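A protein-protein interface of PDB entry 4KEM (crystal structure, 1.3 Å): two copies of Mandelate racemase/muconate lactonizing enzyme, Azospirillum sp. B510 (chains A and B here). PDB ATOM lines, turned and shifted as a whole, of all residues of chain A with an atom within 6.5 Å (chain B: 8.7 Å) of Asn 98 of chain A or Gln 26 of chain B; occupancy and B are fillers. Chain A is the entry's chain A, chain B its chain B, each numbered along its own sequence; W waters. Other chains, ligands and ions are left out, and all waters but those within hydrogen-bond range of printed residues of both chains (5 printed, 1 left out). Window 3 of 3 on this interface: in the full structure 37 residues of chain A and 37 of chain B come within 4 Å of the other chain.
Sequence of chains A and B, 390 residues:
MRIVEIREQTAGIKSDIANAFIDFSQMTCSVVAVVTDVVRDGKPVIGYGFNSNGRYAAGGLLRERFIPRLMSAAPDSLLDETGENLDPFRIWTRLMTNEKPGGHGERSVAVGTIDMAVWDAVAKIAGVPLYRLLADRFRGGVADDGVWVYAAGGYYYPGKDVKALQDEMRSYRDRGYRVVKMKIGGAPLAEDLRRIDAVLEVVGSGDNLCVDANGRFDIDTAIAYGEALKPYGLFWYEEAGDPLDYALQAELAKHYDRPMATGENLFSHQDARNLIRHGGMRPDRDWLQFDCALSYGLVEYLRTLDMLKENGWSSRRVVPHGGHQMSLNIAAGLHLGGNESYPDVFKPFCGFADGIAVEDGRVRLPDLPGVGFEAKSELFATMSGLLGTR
Among the printed residues, merely in contact across the chains: Lys 100 of chain A with Gly 54 of chain B, Asn 98 of chain A with Ile 22 of chain B, Arg 65 of chain A with Tyr 56 of chain B, Glu 99 of chain A with Phe 21 of chain B, Asn 98 of chain A with Gln 26 of chain B, Glu 99 of chain A with Ile 22 of chain B, Arg 65 of chain A with Arg 55 of chain B, Lys 100 of chain A with Ile 22 of chain B and Glu 99 of chain A with Tyr 56 of chain B.
The backbone carbonyl oxygen (O) of Arg 69 of chain A is in hydrogen-bond range of the side-chain hydroxyl (OG) of Ser 72 of chain A (3.1 Å).
The backbone NH (N) of Tyr 56 of chain B sits at hydrogen-bond distance from the side-chain sulfur (SD) of Met 27 of chain B, at 3.6 Å.
Of the 25 printed residues of chain B, 7 touch a printed residue of chain A.
Hydrophobic or aromatic side chains of chain B that line the printed part of chain A: Phe 21, Ile 22 and Tyr 56.
Along chain A the printed residues that touch a printed residue of chain B span positions 65 to 107.
Among the printed residues, 15 pairs touch across the chains.
Among the printed residues, no Asp or Glu carboxylate lies within 4 Å of a Lys or Arg side-chain nitrogen of the other chain.
Asn 98 of chain A touches just these residues of chain B: Ile 22 (3.4 Å), Asp 23 (2.9 Å), Gln 26 (3.6 Å) and Tyr 56 (2.7 Å).
Of chain A, only Arg 69 and Asn 98 come within 4 Å of Gln 26 of chain B.
Of the printed residues of chain A, Gly 54 of chain B touches Lys 100 (3.4 Å).
Printed residues of chain A within 4 Å of Asp 23 of chain B: Asn 98.
Ser 25 of chain B touches none of the printed residues of chain A.
Thr 28 of chain B touches none of the printed residues of chain A.
The nearest printed residue of chain A that does not touch Asp 23 of chain B is Thr 97 of chain A (6.4 Å).
No position is printed for both chains.
OE1 of Gln 26 of chain B sits at hydrogen-bond distance from NE of Arg 69 of chain A (3.0 Å).
NH2 of Arg 69 of chain A is in hydrogen-bond range of OH of Tyr 56 of chain B (3.4 Å).
The side-chain amide oxygen (OD1) of Asn 98 of chain A lies within hydrogen-bond range of the backbone NH (N) of Asp 23 of chain B (2.9 Å).
The backbone carbonyl oxygen (O) of Asn 98 of chain A is in hydrogen-bond range of the side-chain hydroxyl (OH) of Tyr 56 of chain B.
The backbone carbonyl oxygen (O) of Lys 100 of chain A lies within hydrogen-bond range of the guanidinium group (NH2) of Arg 55 of chain B (3.5 Å).
The guanidinium group (NH1) of Arg 107 of chain A lies close to the guanidinium group (NH2) of Arg 55 of chain B, at 3.4 Å.
Water W5 lies within hydrogen-bond range of the backbone NH of Lys 100 of chain A (2.9 Å) and the backbone carbonyl oxygen of Gly 54 of chain B (2.9 Å).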
ATOM      1  N   ARG A  65      19.117 -10.762  32.448  1.00  0.00           N
ATOM      2  CA  ARG A  65      18.736  -9.798  31.424  1.00  0.00           C
ATOM      3  C   ARG A  65      17.617  -8.849  31.860  1.00  0.00           C
ATOM      4  O   ARG A  65      17.768  -7.623  31.852  1.00  0.00           O
ATOM      5  CB  ARG A  65      18.303 -10.525  30.148  1.00  0.00           C
ATOM      6  CG  ARG A  65      19.392 -11.418  29.533  1.00  0.00           C
ATOM      7  CD  ARG A  65      19.679 -11.079  28.075  1.00  0.00           C
ATOM      8  NE  ARG A  65      18.591 -11.390  27.143  1.00  0.00           N
ATOM      9  CZ  ARG A  65      18.364 -12.584  26.603  1.00  0.00           C
ATOM     10  NH1 ARG A  65      17.387 -12.730  25.731  1.00  0.00           N
ATOM     11  NH2 ARG A  65      19.105 -13.646  26.914  1.00  0.00           N
ATOM     12  N   ARG A  69      17.425  -4.660  33.624  1.00  0.00           N
ATOM     13  CA  ARG A  69      16.962  -3.605  32.736  1.00  0.00           C
ATOM     14  C   ARG A  69      15.949  -2.683  33.362  1.00  0.00           C
ATOM     15  O   ARG A  69      16.063  -1.465  33.252  1.00  0.00           O
ATOM     16  CB  ARG A  69      16.346  -4.202  31.490  1.00  0.00           C
ATOM     17  CG  ARG A  69      17.254  -4.116  30.342  1.00  0.00           C
ATOM     18  CD  ARG A  69      16.699  -4.828  29.135  1.00  0.00           C
ATOM     19  NE  ARG A  69      17.778  -5.469  28.404  1.00  0.00           N
ATOM     20  CZ  ARG A  69      17.655  -6.597  27.714  1.00  0.00           C
ATOM     21  NH1 ARG A  69      16.503  -7.235  27.679  1.00  0.00           N
ATOM     22  NH2 ARG A  69      18.694  -7.110  27.079  1.00  0.00           N
ATOM     23  N   SER A  72      17.402  -0.602  36.313  1.00  0.00           N
ATOM     24  CA  SER A  72      18.341   0.457  35.953  1.00  0.00           C
ATOM     25  C   SER A  72      17.643   1.650  35.289  1.00  0.00           C
ATOM     26  O   SER A  72      18.265   2.689  35.070  1.00  0.00           O
ATOM     27  CB  SER A  72      19.447  -0.085  35.046  1.00  0.00           C
ATOM     28  OG  SER A  72      18.921  -0.548  33.824  1.00  0.00           O
ATOM     29  N   THR A  93       8.438  -2.014  26.868  1.00  0.00           N
ATOM     30  CA  THR A  93       9.443  -1.460  25.980  1.00  0.00           C
ATOM     31  C   THR A  93      10.816  -1.494  26.638  1.00  0.00           C
ATOM     32  O   THR A  93      11.796  -1.854  25.993  1.00  0.00           O
ATOM     33  CB  THR A  93       9.052  -0.045  25.542  1.00  0.00           C
ATOM     34  OG1 THR A  93       7.843  -0.125  24.779  1.00  0.00           O
ATOM     35  CG2 THR A  93      10.150   0.607  24.686  1.00  0.00           C
ATOM     36  N   ARG A  94      10.908  -1.154  27.922  1.00  0.00           N
ATOM     37  CA  ARG A  94      12.187  -1.170  28.598  1.00  0.00           C
ATOM     38  C   ARG A  94      12.718  -2.594  28.697  1.00  0.00           C
ATOM     39  O   ARG A  94      13.910  -2.834  28.461  1.00  0.00           O
ATOM     40  CB  ARG A  94      12.066  -0.529  29.983  1.00  0.00           C
ATOM     41  CG  ARG A  94      13.358  -0.538  30.799  1.00  0.00           C
ATOM     42  CD  ARG A  94      14.461   0.343  30.196  1.00  0.00           C
ATOM     43  NE  ARG A  94      15.620   0.414  31.085  1.00  0.00           N
ATOM     44  CZ  ARG A  94      16.608   1.297  30.962  1.00  0.00           C
ATOM     45  NH1 ARG A  94      16.589   2.201  29.987  1.00  0.00           N
ATOM     46  NH2 ARG A  94      17.615   1.288  31.826  1.00  0.00           N
ATOM     47  N   LEU A  95      11.841  -3.547  28.981  1.00  0.00           N
ATOM     48  CA  LEU A  95      12.251  -4.934  29.137  1.00  0.00           C
ATOM     49  C   LEU A  95      12.854  -5.460  27.834  1.00  0.00           C
ATOM     50  O   LEU A  95      13.803  -6.248  27.847  1.00  0.00           O
ATOM     51  CB  LEU A  95      11.055  -5.826  29.526  1.00  0.00           C
ATOM     52  CG  LEU A  95      10.667  -5.761  31.003  1.00  0.00           C
ATOM     53  CD1 LEU A  95       9.301  -6.314  31.200  1.00  0.00           C
ATOM     54  CD2 LEU A  95      11.694  -6.496  31.867  1.00  0.00           C
ATOM     55  N   MET A  96      12.301  -5.041  26.707  1.00  0.00           N
ATOM     56  CA  MET A  96      12.683  -5.623  25.423  1.00  0.00           C
ATOM     57  C   MET A  96      13.701  -4.809  24.659  1.00  0.00           C
ATOM     58  O   MET A  96      14.038  -5.124  23.508  1.00  0.00           O
ATOM     59  CB  MET A  96      11.449  -5.858  24.570  1.00  0.00           C
ATOM     60  CG  MET A  96      10.608  -6.991  25.127  1.00  0.00           C
ATOM     61  SD  MET A  96      11.453  -8.598  25.172  1.00  0.00           S
ATOM     62  CE  MET A  96      11.549  -8.896  23.408  1.00  0.00           C
ATOM     63  N   THR A  97      14.244  -3.786  25.300  1.00  0.00           N
ATOM     64  CA  THR A  97      15.299  -3.009  24.686  1.00  0.00           C
ATOM     65  C   THR A  97      16.581  -3.838  24.523  1.00  0.00           C
ATOM     66  O   THR A  97      17.020  -4.526  25.446  1.00  0.00           O
ATOM     67  CB  THR A  97      15.536  -1.726  25.488  1.00  0.00           C
ATOM     68  OG1 THR A  97      14.411  -0.855  25.317  1.00  0.00           O
ATOM     69  CG2 THR A  97      16.795  -1.004  25.037  1.00  0.00           C
ATOM     70  N   ASN A  98      17.167  -3.754  23.331  1.00  0.00           N
ATOM     71  CA  ASN A  98      18.350  -4.526  22.952  1.00  0.00           C
ATOM     72  C   ASN A  98      18.103  -6.041  22.807  1.00  0.00           C
ATOM     73  O   ASN A  98      19.040  -6.847  22.898  1.00  0.00           O
ATOM     74  CB  ASN A  98      19.533  -4.204  23.851  1.00  0.00           C
ATOM     75  CG  ASN A  98      19.968  -2.791  23.703  1.00  0.00           C
ATOM     76  OD1 ASN A  98      19.956  -2.242  22.605  1.00  0.00           O
ATOM     77  ND2 ASN A  98      20.368  -2.181  24.807  1.00  0.00           N
ATOM     78  N   GLU A  99      16.867  -6.423  22.522  1.00  0.00           N
ATOM     79  CA  GLU A  99      16.519  -7.809  22.188  1.00  0.00           C
ATOM     80  C   GLU A  99      16.290  -7.945  20.683  1.00  0.00           C
ATOM     81  O   GLU A  99      15.510  -7.198  20.086  1.00  0.00           O
ATOM     82  CB  GLU A  99      15.274  -8.224  22.947  1.00  0.00           C
ATOM     83  CG  GLU A  99      15.493  -8.307  24.446  1.00  0.00           C
ATOM     84  CD  GLU A  99      16.310  -9.495  24.885  1.00  0.00           C
ATOM     85  OE1 GLU A  99      16.221 -10.576  24.255  1.00  0.00           O
ATOM     86  OE2 GLU A  99      17.020  -9.363  25.903  1.00  0.00           O
ATOM     87  N   LYS A 100      17.006  -8.875  20.053  1.00  0.00           N
ATOM     88  CA  LYS A 100      16.835  -9.075  18.622  1.00  0.00           C
ATOM     89  C   LYS A 100      15.533  -9.791  18.324  1.00  0.00           C
ATOM     90  O   LYS A 100      15.003 -10.497  19.164  1.00  0.00           O
ATOM     91  CB  LYS A 100      18.019  -9.857  18.016  1.00  0.00           C
ATOM     92  CG  LYS A 100      19.247  -9.004  17.783  1.00  0.00           C
ATOM     93  CD  LYS A 100      20.406  -9.843  17.266  1.00  0.00           C
ATOM     94  CE  LYS A 100      20.218 -10.220  15.823  1.00  0.00           C
ATOM     95  NZ  LYS A 100      21.395 -10.977  15.266  1.00  0.00           N
ATOM     96  N   ARG A 107      12.691 -16.437  26.843  1.00  0.00           N
ATOM     97  CA  ARG A 107      12.611 -15.024  27.229  1.00  0.00           C
ATOM     98  C   ARG A 107      11.149 -14.548  27.200  1.00  0.00           C
ATOM     99  O   ARG A 107      10.782 -13.624  27.933  1.00  0.00           O
ATOM    100  CB  ARG A 107      13.528 -14.136  26.363  1.00  0.00           C
ATOM    101  CG  ARG A 107      13.133 -14.098  24.899  1.00  0.00           C
ATOM    102  CD  ARG A 107      13.847 -12.958  24.168  1.00  0.00           C
ATOM    103  NE  ARG A 107      13.256 -12.748  22.852  1.00  0.00           N
ATOM    104  CZ  ARG A 107      13.813 -12.078  21.853  1.00  0.00           C
ATOM    105  NH1 ARG A 107      15.027 -11.551  21.969  1.00  0.00           N
ATOM    106  NH2 ARG A 107      13.162 -12.014  20.688  1.00  0.00           N
ATOM    107  N   THR B  10      30.004 -17.569  31.375  1.00  0.00           N
ATOM    108  CA  THR B  10      29.535 -16.452  30.571  1.00  0.00           C
ATOM    109  C   THR B  10      30.681 -15.482  30.275  1.00  0.00           C
ATOM    110  O   THR B  10      31.451 -15.138  31.168  1.00  0.00           O
ATOM    111  CB  THR B  10      28.392 -15.719  31.285  1.00  0.00           C
ATOM    112  OG1 THR B  10      27.330 -16.653  31.539  1.00  0.00           O
ATOM    113  CG2 THR B  10      27.873 -14.571  30.424  1.00  0.00           C
ATOM    114  N   ALA B  11      30.792 -15.087  29.016  1.00  0.00           N
ATOM    115  CA  ALA B  11      31.783 -14.106  28.575  1.00  0.00           C
ATOM    116  C   ALA B  11      31.082 -12.829  28.141  1.00  0.00           C
ATOM    117  O   ALA B  11      29.959 -12.870  27.658  1.00  0.00           O
ATOM    118  CB  ALA B  11      32.599 -14.660  27.417  1.00  0.00           C
ATOM    119  N   GLY B  12      31.760 -11.700  28.311  1.00  0.00           N
ATOM    120  CA  GLY B  12      31.278 -10.423  27.823  1.00  0.00           C
ATOM    121  C   GLY B  12      31.837 -10.125  26.441  1.00  0.00           C
ATOM    122  O   GLY B  12      33.030 -10.319  26.186  1.00  0.00           O
ATOM    123  N   ILE B  13      30.966  -9.677  25.539  1.00  0.00           N
ATOM    124  CA  ILE B  13      31.366  -9.095  24.255  1.00  0.00           C
ATOM    125  C   ILE B  13      30.654  -7.743  24.073  1.00  0.00           C
ATOM    126  O   ILE B  13      30.035  -7.463  23.050  1.00  0.00           O
ATOM    127  CB  ILE B  13      31.084 -10.048  23.066  1.00  0.00           C
ATOM    128  CG1 ILE B  13      29.706 -10.698  23.163  1.00  0.00           C
ATOM    129  CG2 ILE B  13      32.145 -11.155  23.013  1.00  0.00           C
ATOM    130  CD1 ILE B  13      29.303 -11.411  21.868  1.00  0.00           C
ATOM    131  N   LYS B  14      30.754  -6.925  25.103  1.00  0.00           N
ATOM    132  CA  LYS B  14      30.010  -5.674  25.175  1.00  0.00           C
ATOM    133  C   LYS B  14      30.712  -4.557  24.428  1.00  0.00           C
ATOM    134  O   LYS B  14      31.931  -4.432  24.485  1.00  0.00           O
ATOM    135  CB  LYS B  14      29.874  -5.271  26.643  1.00  0.00           C
ATOM    136  CG  LYS B  14      29.083  -6.266  27.479  1.00  0.00           C
ATOM    137  CD  LYS B  14      28.952  -5.836  28.930  1.00  0.00           C
ATOM    138  CE  LYS B  14      28.258  -6.922  29.749  1.00  0.00           C
ATOM    139  NZ  LYS B  14      28.073  -6.548  31.176  1.00  0.00           N
ATOM    140  N   SER B  15      29.932  -3.733  23.739  1.00  0.00           N
ATOM    141  CA  SER B  15      30.440  -2.484  23.193  1.00  0.00           C
ATOM    142  C   SER B  15      29.244  -1.661  22.721  1.00  0.00           C
ATOM    143  O   SER B  15      28.120  -2.161  22.640  1.00  0.00           O
ATOM    144  CB  SER B  15      31.396  -2.730  22.040  1.00  0.00           C
ATOM    145  OG  SER B  15      30.687  -2.910  20.836  1.00  0.00           O
ATOM    146  N   ASP B  16      29.506  -0.410  22.380  1.00  0.00           N
ATOM    147  CA  ASP B  16      28.445   0.496  21.960  1.00  0.00           C
ATOM    148  C   ASP B  16      28.158   0.460  20.451  1.00  0.00           C
ATOM    149  O   ASP B  16      27.411   1.297  19.952  1.00  0.00           O
ATOM    150  CB  ASP B  16      28.749   1.917  22.433  1.00  0.00           C
ATOM    151  CG  ASP B  16      28.610   2.073  23.934  1.00  0.00           C
ATOM    152  OD1 ASP B  16      27.863   1.298  24.569  1.00  0.00           O
ATOM    153  OD2 ASP B  16      29.225   3.003  24.484  1.00  0.00           O
ATOM    154  N   ILE B  17      28.690  -0.517  19.717  1.00  0.00           N
ATOM    155  CA  ILE B  17      28.258  -0.672  18.341  1.00  0.00           C
ATOM    156  C   ILE B  17      26.761  -0.966  18.317  1.00  0.00           C
ATOM    157  O   ILE B  17      26.192  -1.537  19.260  1.00  0.00           O
ATOM    158  CB  ILE B  17      29.046  -1.782  17.575  1.00  0.00           C
ATOM    159  CG1 ILE B  17      28.823  -3.172  18.190  1.00  0.00           C
ATOM    160  CG2 ILE B  17      30.533  -1.430  17.513  1.00  0.00           C
ATOM    161  CD1 ILE B  17      29.502  -4.309  17.422  1.00  0.00           C
ATOM    162  N   ALA B  18      26.123  -0.589  17.213  1.00  0.00           N
ATOM    163  CA  ALA B  18      24.678  -0.718  17.081  1.00  0.00           C
ATOM    164  C   ALA B  18      24.307  -1.031  15.644  1.00  0.00           C
ATOM    165  O   ALA B  18      24.990  -0.615  14.700  1.00  0.00           O
ATOM    166  CB  ALA B  18      23.980   0.573  17.517  1.00  0.00           C
ATOM    167  N   ASN B  19      23.261  -1.832  15.478  1.00  0.00           N
ATOM    168  CA  ASN B  19      22.619  -2.029  14.187  1.00  0.00           C
ATOM    169  C   ASN B  19      21.240  -1.367  14.238  1.00  0.00           C
ATOM    170  O   ASN B  19      20.967  -0.615  15.173  1.00  0.00           O
ATOM    171  CB  ASN B  19      22.601  -3.526  13.808  1.00  0.00           C
ATOM    172  CG  ASN B  19      21.798  -4.380  14.769  1.00  0.00           C
ATOM    173  OD1 ASN B  19      20.741  -3.975  15.219  1.00  0.00           O
ATOM    174  ND2 ASN B  19      22.297  -5.592  15.069  1.00  0.00           N
ATOM    175  N   ALA B  20      20.376  -1.610  13.254  1.00  0.00           N
ATOM    176  CA  ALA B  20      19.094  -0.928  13.221  1.00  0.00           C
ATOM    177  C   ALA B  20      18.156  -1.332  14.341  1.00  0.00           C
ATOM    178  O   ALA B  20      17.198  -0.609  14.626  1.00  0.00           O
ATOM    179  CB  ALA B  20      18.431  -1.135  11.870  1.00  0.00           C
ATOM    180  N   PHE B  21      18.415  -2.485  14.951  1.00  0.00           N
ATOM    181  CA  PHE B  21      17.483  -3.040  15.934  1.00  0.00           C
ATOM    182  C   PHE B  21      17.961  -2.932  17.385  1.00  0.00           C
ATOM    183  O   PHE B  21      17.160  -2.617  18.261  1.00  0.00           O
ATOM    184  CB  PHE B  21      17.191  -4.507  15.619  1.00  0.00           C
ATOM    185  CG  PHE B  21      15.760  -4.917  15.880  1.00  0.00           C
ATOM    186  CD1 PHE B  21      15.298  -5.134  17.170  1.00  0.00           C
ATOM    187  CD2 PHE B  21      14.883  -5.096  14.828  1.00  0.00           C
ATOM    188  CE1 PHE B  21      13.967  -5.511  17.412  1.00  0.00           C
ATOM    189  CE2 PHE B  21      13.561  -5.463  15.045  1.00  0.00           C
ATOM    190  CZ  PHE B  21      13.104  -5.672  16.339  1.00  0.00           C
ATOM    191  N   ILE B  22      19.249  -3.189  17.635  1.00  0.00           N
ATOM    192  CA  ILE B  22      19.814  -3.212  18.994  1.00  0.00           C
ATOM    193  C   ILE B  22      21.193  -2.554  19.045  1.00  0.00           C
ATOM    194  O   ILE B  22      21.858  -2.392  17.997  1.00  0.00           O
ATOM    195  CB  ILE B  22      19.973  -4.670  19.570  1.00  0.00           C
ATOM    196  CG1 ILE B  22      21.110  -5.435  18.896  1.00  0.00           C
ATOM    197  CG2 ILE B  22      18.669  -5.438  19.493  1.00  0.00           C
ATOM    198  CD1 ILE B  22      21.573  -6.616  19.730  1.00  0.00           C
ATOM    199  N   ASP B  23      21.650  -2.227  20.253  1.00  0.00           N
ATOM    200  CA  ASP B  23      23.075  -2.005  20.480  1.00  0.00           C
ATOM    201  C   ASP B  23      23.645  -3.150  21.319  1.00  0.00           C
ATOM    202  O   ASP B  23      22.886  -3.980  21.847  1.00  0.00           O
ATOM    203  CB  ASP B  23      23.375  -0.598  21.035  1.00  0.00           C
ATOM    204  CG  ASP B  23      23.085  -0.433  22.523  1.00  0.00           C
ATOM    205  OD1 ASP B  23      23.386  -1.321  23.331  1.00  0.00           O
ATOM    206  OD2 ASP B  23      22.564   0.648  22.910  1.00  0.00           O
ATOM    207  N   PHE B  24      24.970  -3.213  21.400  1.00  0.00           N
ATOM    208  CA  PHE B  24      25.651  -4.378  21.948  1.00  0.00           C
ATOM    209  C   PHE B  24      26.222  -4.103  23.344  1.00  0.00           C
ATOM    210  O   PHE B  24      27.057  -4.855  23.843  1.00  0.00           O
ATOM    211  CB  PHE B  24      26.691  -4.889  20.936  1.00  0.00           C
ATOM    212  CG  PHE B  24      26.073  -5.586  19.778  1.00  0.00           C
ATOM    213  CD1 PHE B  24      25.404  -4.892  18.789  1.00  0.00           C
ATOM    214  CD2 PHE B  24      26.111  -6.966  19.714  1.00  0.00           C
ATOM    215  CE1 PHE B  24      24.817  -5.563  17.744  1.00  0.00           C
ATOM    216  CE2 PHE B  24      25.530  -7.634  18.672  1.00  0.00           C
ATOM    217  CZ  PHE B  24      24.881  -6.942  17.699  1.00  0.00           C
ATOM    218  N   SER B  25      25.685  -3.075  24.011  1.00  0.00           N
ATOM    219  CA  SER B  25      26.238  -2.614  25.284  1.00  0.00           C
ATOM    220  C   SER B  25      26.124  -3.637  26.418  1.00  0.00           C
ATOM    221  O   SER B  25      26.800  -3.513  27.428  1.00  0.00           O
ATOM    222  CB  SER B  25      25.574  -1.302  25.693  1.00  0.00           C
ATOM    223  OG  SER B  25      24.177  -1.459  25.892  1.00  0.00           O
ATOM    224  N   GLN B  26      25.236  -4.609  26.257  1.00  0.00           N
ATOM    225  CA  GLN B  26      25.031  -5.638  27.268  1.00  0.00           C
ATOM    226  C   GLN B  26      25.371  -7.043  26.743  1.00  0.00           C
ATOM    227  O   GLN B  26      25.111  -8.048  27.416  1.00  0.00           O
ATOM    228  CB  GLN B  26      23.561  -5.618  27.742  1.00  0.00           C
ATOM    229  CG  GLN B  26      23.026  -4.248  28.234  1.00  0.00           C
ATOM    230  CD  GLN B  26      21.485  -4.150  28.234  1.00  0.00           C
ATOM    231  OE1 GLN B  26      20.780  -5.158  28.223  1.00  0.00           O
ATOM    232  NE2 GLN B  26      20.970  -2.921  28.244  1.00  0.00           N
ATOM    233  N   MET B  27      25.952  -7.130  25.552  1.00  0.00           N
ATOM    234  CA  MET B  27      26.048  -8.426  24.885  1.00  0.00           C
ATOM    235  C   MET B  27      27.023  -9.390  25.559  1.00  0.00           C
ATOM    236  O   MET B  27      28.143  -9.021  25.939  1.00  0.00           O
ATOM    237  CB  MET B  27      26.440  -8.264  23.423  1.00  0.00           C
ATOM    238  CG  MET B  27      26.190  -9.495  22.574  1.00  0.00           C
ATOM    239  SD  MET B  27      24.504 -10.153  22.596  1.00  0.00           S
ATOM    240  CE  MET B  27      23.568  -8.701  22.099  1.00  0.00           C
ATOM    241  N   THR B  28      26.565 -10.632  25.697  1.00  0.00           N
ATOM    242  CA  THR B  28      27.322 -11.716  26.315  1.00  0.00           C
ATOM    243  C   THR B  28      27.246 -12.955  25.419  1.00  0.00           C
ATOM    244  O   THR B  28      26.506 -12.967  24.436  1.00  0.00           O
ATOM    245  CB  THR B  28      26.715 -12.080  27.663  1.00  0.00           C
ATOM    246  OG1 THR B  28      25.337 -12.438  27.460  1.00  0.00           O
ATOM    247  CG2 THR B  28      26.820 -10.899  28.651  1.00  0.00           C
ATOM    248  N   CYS B  29      28.028 -13.980  25.740  1.00  0.00           N
ATOM    249  CA  CYS B  29      27.879 -15.292  25.110  1.00  0.00           C
ATOM    250  C   CYS B  29      28.293 -16.362  26.109  1.00  0.00           C
ATOM    251  O   CYS B  29      29.033 -16.098  27.074  1.00  0.00           O
ATOM    252  CB  CYS B  29      28.705 -15.395  23.819  1.00  0.00           C
ATOM    253  SG  CYS B  29      30.509 -15.325  24.016  1.00  0.00           S
ATOM    254  N   GLY B  54      24.706 -11.675  19.537  1.00  0.00           N
ATOM    255  CA  GLY B  54      23.381 -11.136  19.271  1.00  0.00           C
ATOM    256  C   GLY B  54      22.252 -11.710  20.091  1.00  0.00           C
ATOM    257  O   GLY B  54      21.244 -11.038  20.309  1.00  0.00           O
ATOM    258  N   ARG B  55      22.406 -12.947  20.538  1.00  0.00           N
ATOM    259  CA  ARG B  55      21.369 -13.593  21.318  1.00  0.00           C
ATOM    260  C   ARG B  55      21.636 -13.675  22.828  1.00  0.00           C
ATOM    261  O   ARG B  55      20.735 -14.103  23.567  1.00  0.00           O
ATOM    262  CB  ARG B  55      21.105 -15.006  20.796  1.00  0.00           C
ATOM    263  CG  ARG B  55      20.705 -15.105  19.319  1.00  0.00           C
ATOM    264  CD  ARG B  55      19.718 -14.063  18.817  1.00  0.00           C
ATOM    265  NE  ARG B  55      18.439 -14.106  19.500  1.00  0.00           N
ATOM    266  CZ  ARG B  55      17.302 -13.690  18.947  1.00  0.00           C
ATOM    267  NH1 ARG B  55      17.273 -13.229  17.706  1.00  0.00           N
ATOM    268  NH2 ARG B  55      16.174 -13.723  19.641  1.00  0.00           N
ATOM    269  N   TYR B  56      22.814 -13.232  23.271  1.00  0.00           N
ATOM    270  CA  TYR B  56      23.262 -13.277  24.663  1.00  0.00           C
ATOM    271  C   TYR B  56      23.628 -14.713  25.069  1.00  0.00           C
ATOM    272  O   TYR B  56      23.364 -15.685  24.364  1.00  0.00           O
ATOM    273  CB  TYR B  56      22.224 -12.669  25.624  1.00  0.00           C
ATOM    274  CG  TYR B  56      21.899 -11.206  25.361  1.00  0.00           C
ATOM    275  CD1 TYR B  56      22.629 -10.193  25.964  1.00  0.00           C
ATOM    276  CD2 TYR B  56      20.854 -10.848  24.504  1.00  0.00           C
ATOM    277  CE1 TYR B  56      22.326  -8.860  25.731  1.00  0.00           C
ATOM    278  CE2 TYR B  56      20.552  -9.526  24.263  1.00  0.00           C
ATOM    279  CZ  TYR B  56      21.305  -8.541  24.876  1.00  0.00           C
ATOM    280  OH  TYR B  56      21.064  -7.201  24.662  1.00  0.00           O
ATOM    281  N   ALA B  57      24.212 -14.829  26.253  1.00  0.00           N
ATOM    282  CA  ALA B  57      24.571 -16.114  26.815  1.00  0.00           C
ATOM    283  C   ALA B  57      23.292 -16.885  27.185  1.00  0.00           C
ATOM    284  O   ALA B  57      22.218 -16.303  27.421  1.00  0.00           O
ATOM    285  CB  ALA B  57      25.409 -15.892  28.044  1.00  0.00           C
ATOM    286  N   ARG B 216      14.492  -4.651  10.811  1.00  0.00           N
ATOM    287  CA  ARG B 216      13.852  -3.470  11.398  1.00  0.00           C
ATOM    288  C   ARG B 216      12.709  -2.870  10.566  1.00  0.00           C
ATOM    289  O   ARG B 216      11.870  -2.170  11.132  1.00  0.00           O
ATOM    290  CB  ARG B 216      14.931  -2.402  11.690  1.00  0.00           C
ATOM    291  CG  ARG B 216      14.445  -1.104  12.399  1.00  0.00           C
ATOM    292  CD  ARG B 216      13.951  -1.338  13.824  1.00  0.00           C
ATOM    293  NE  ARG B 216      12.628  -1.946  13.876  1.00  0.00           N
ATOM    294  CZ  ARG B 216      11.996  -2.305  14.991  1.00  0.00           C
ATOM    295  NH1 ARG B 216      10.799  -2.863  14.905  1.00  0.00           N
ATOM    296  NH2 ARG B 216      12.566  -2.148  16.181  1.00  0.00           N
HETATM  297  O   HOH W   1      21.019  -7.734  29.242  1.00  0.00           O
HETATM  298  O   HOH W   2      16.415  -2.216  20.971  1.00  0.00           O
HETATM  299  O   HOH W   3      21.125   0.671  25.145  1.00  0.00           O
HETATM  300  O   HOH W   4      21.452 -14.027  28.783  1.00  0.00           O
HETATM  301  O   HOH W   5      18.566 -10.885  21.413  1.00  0.00           O
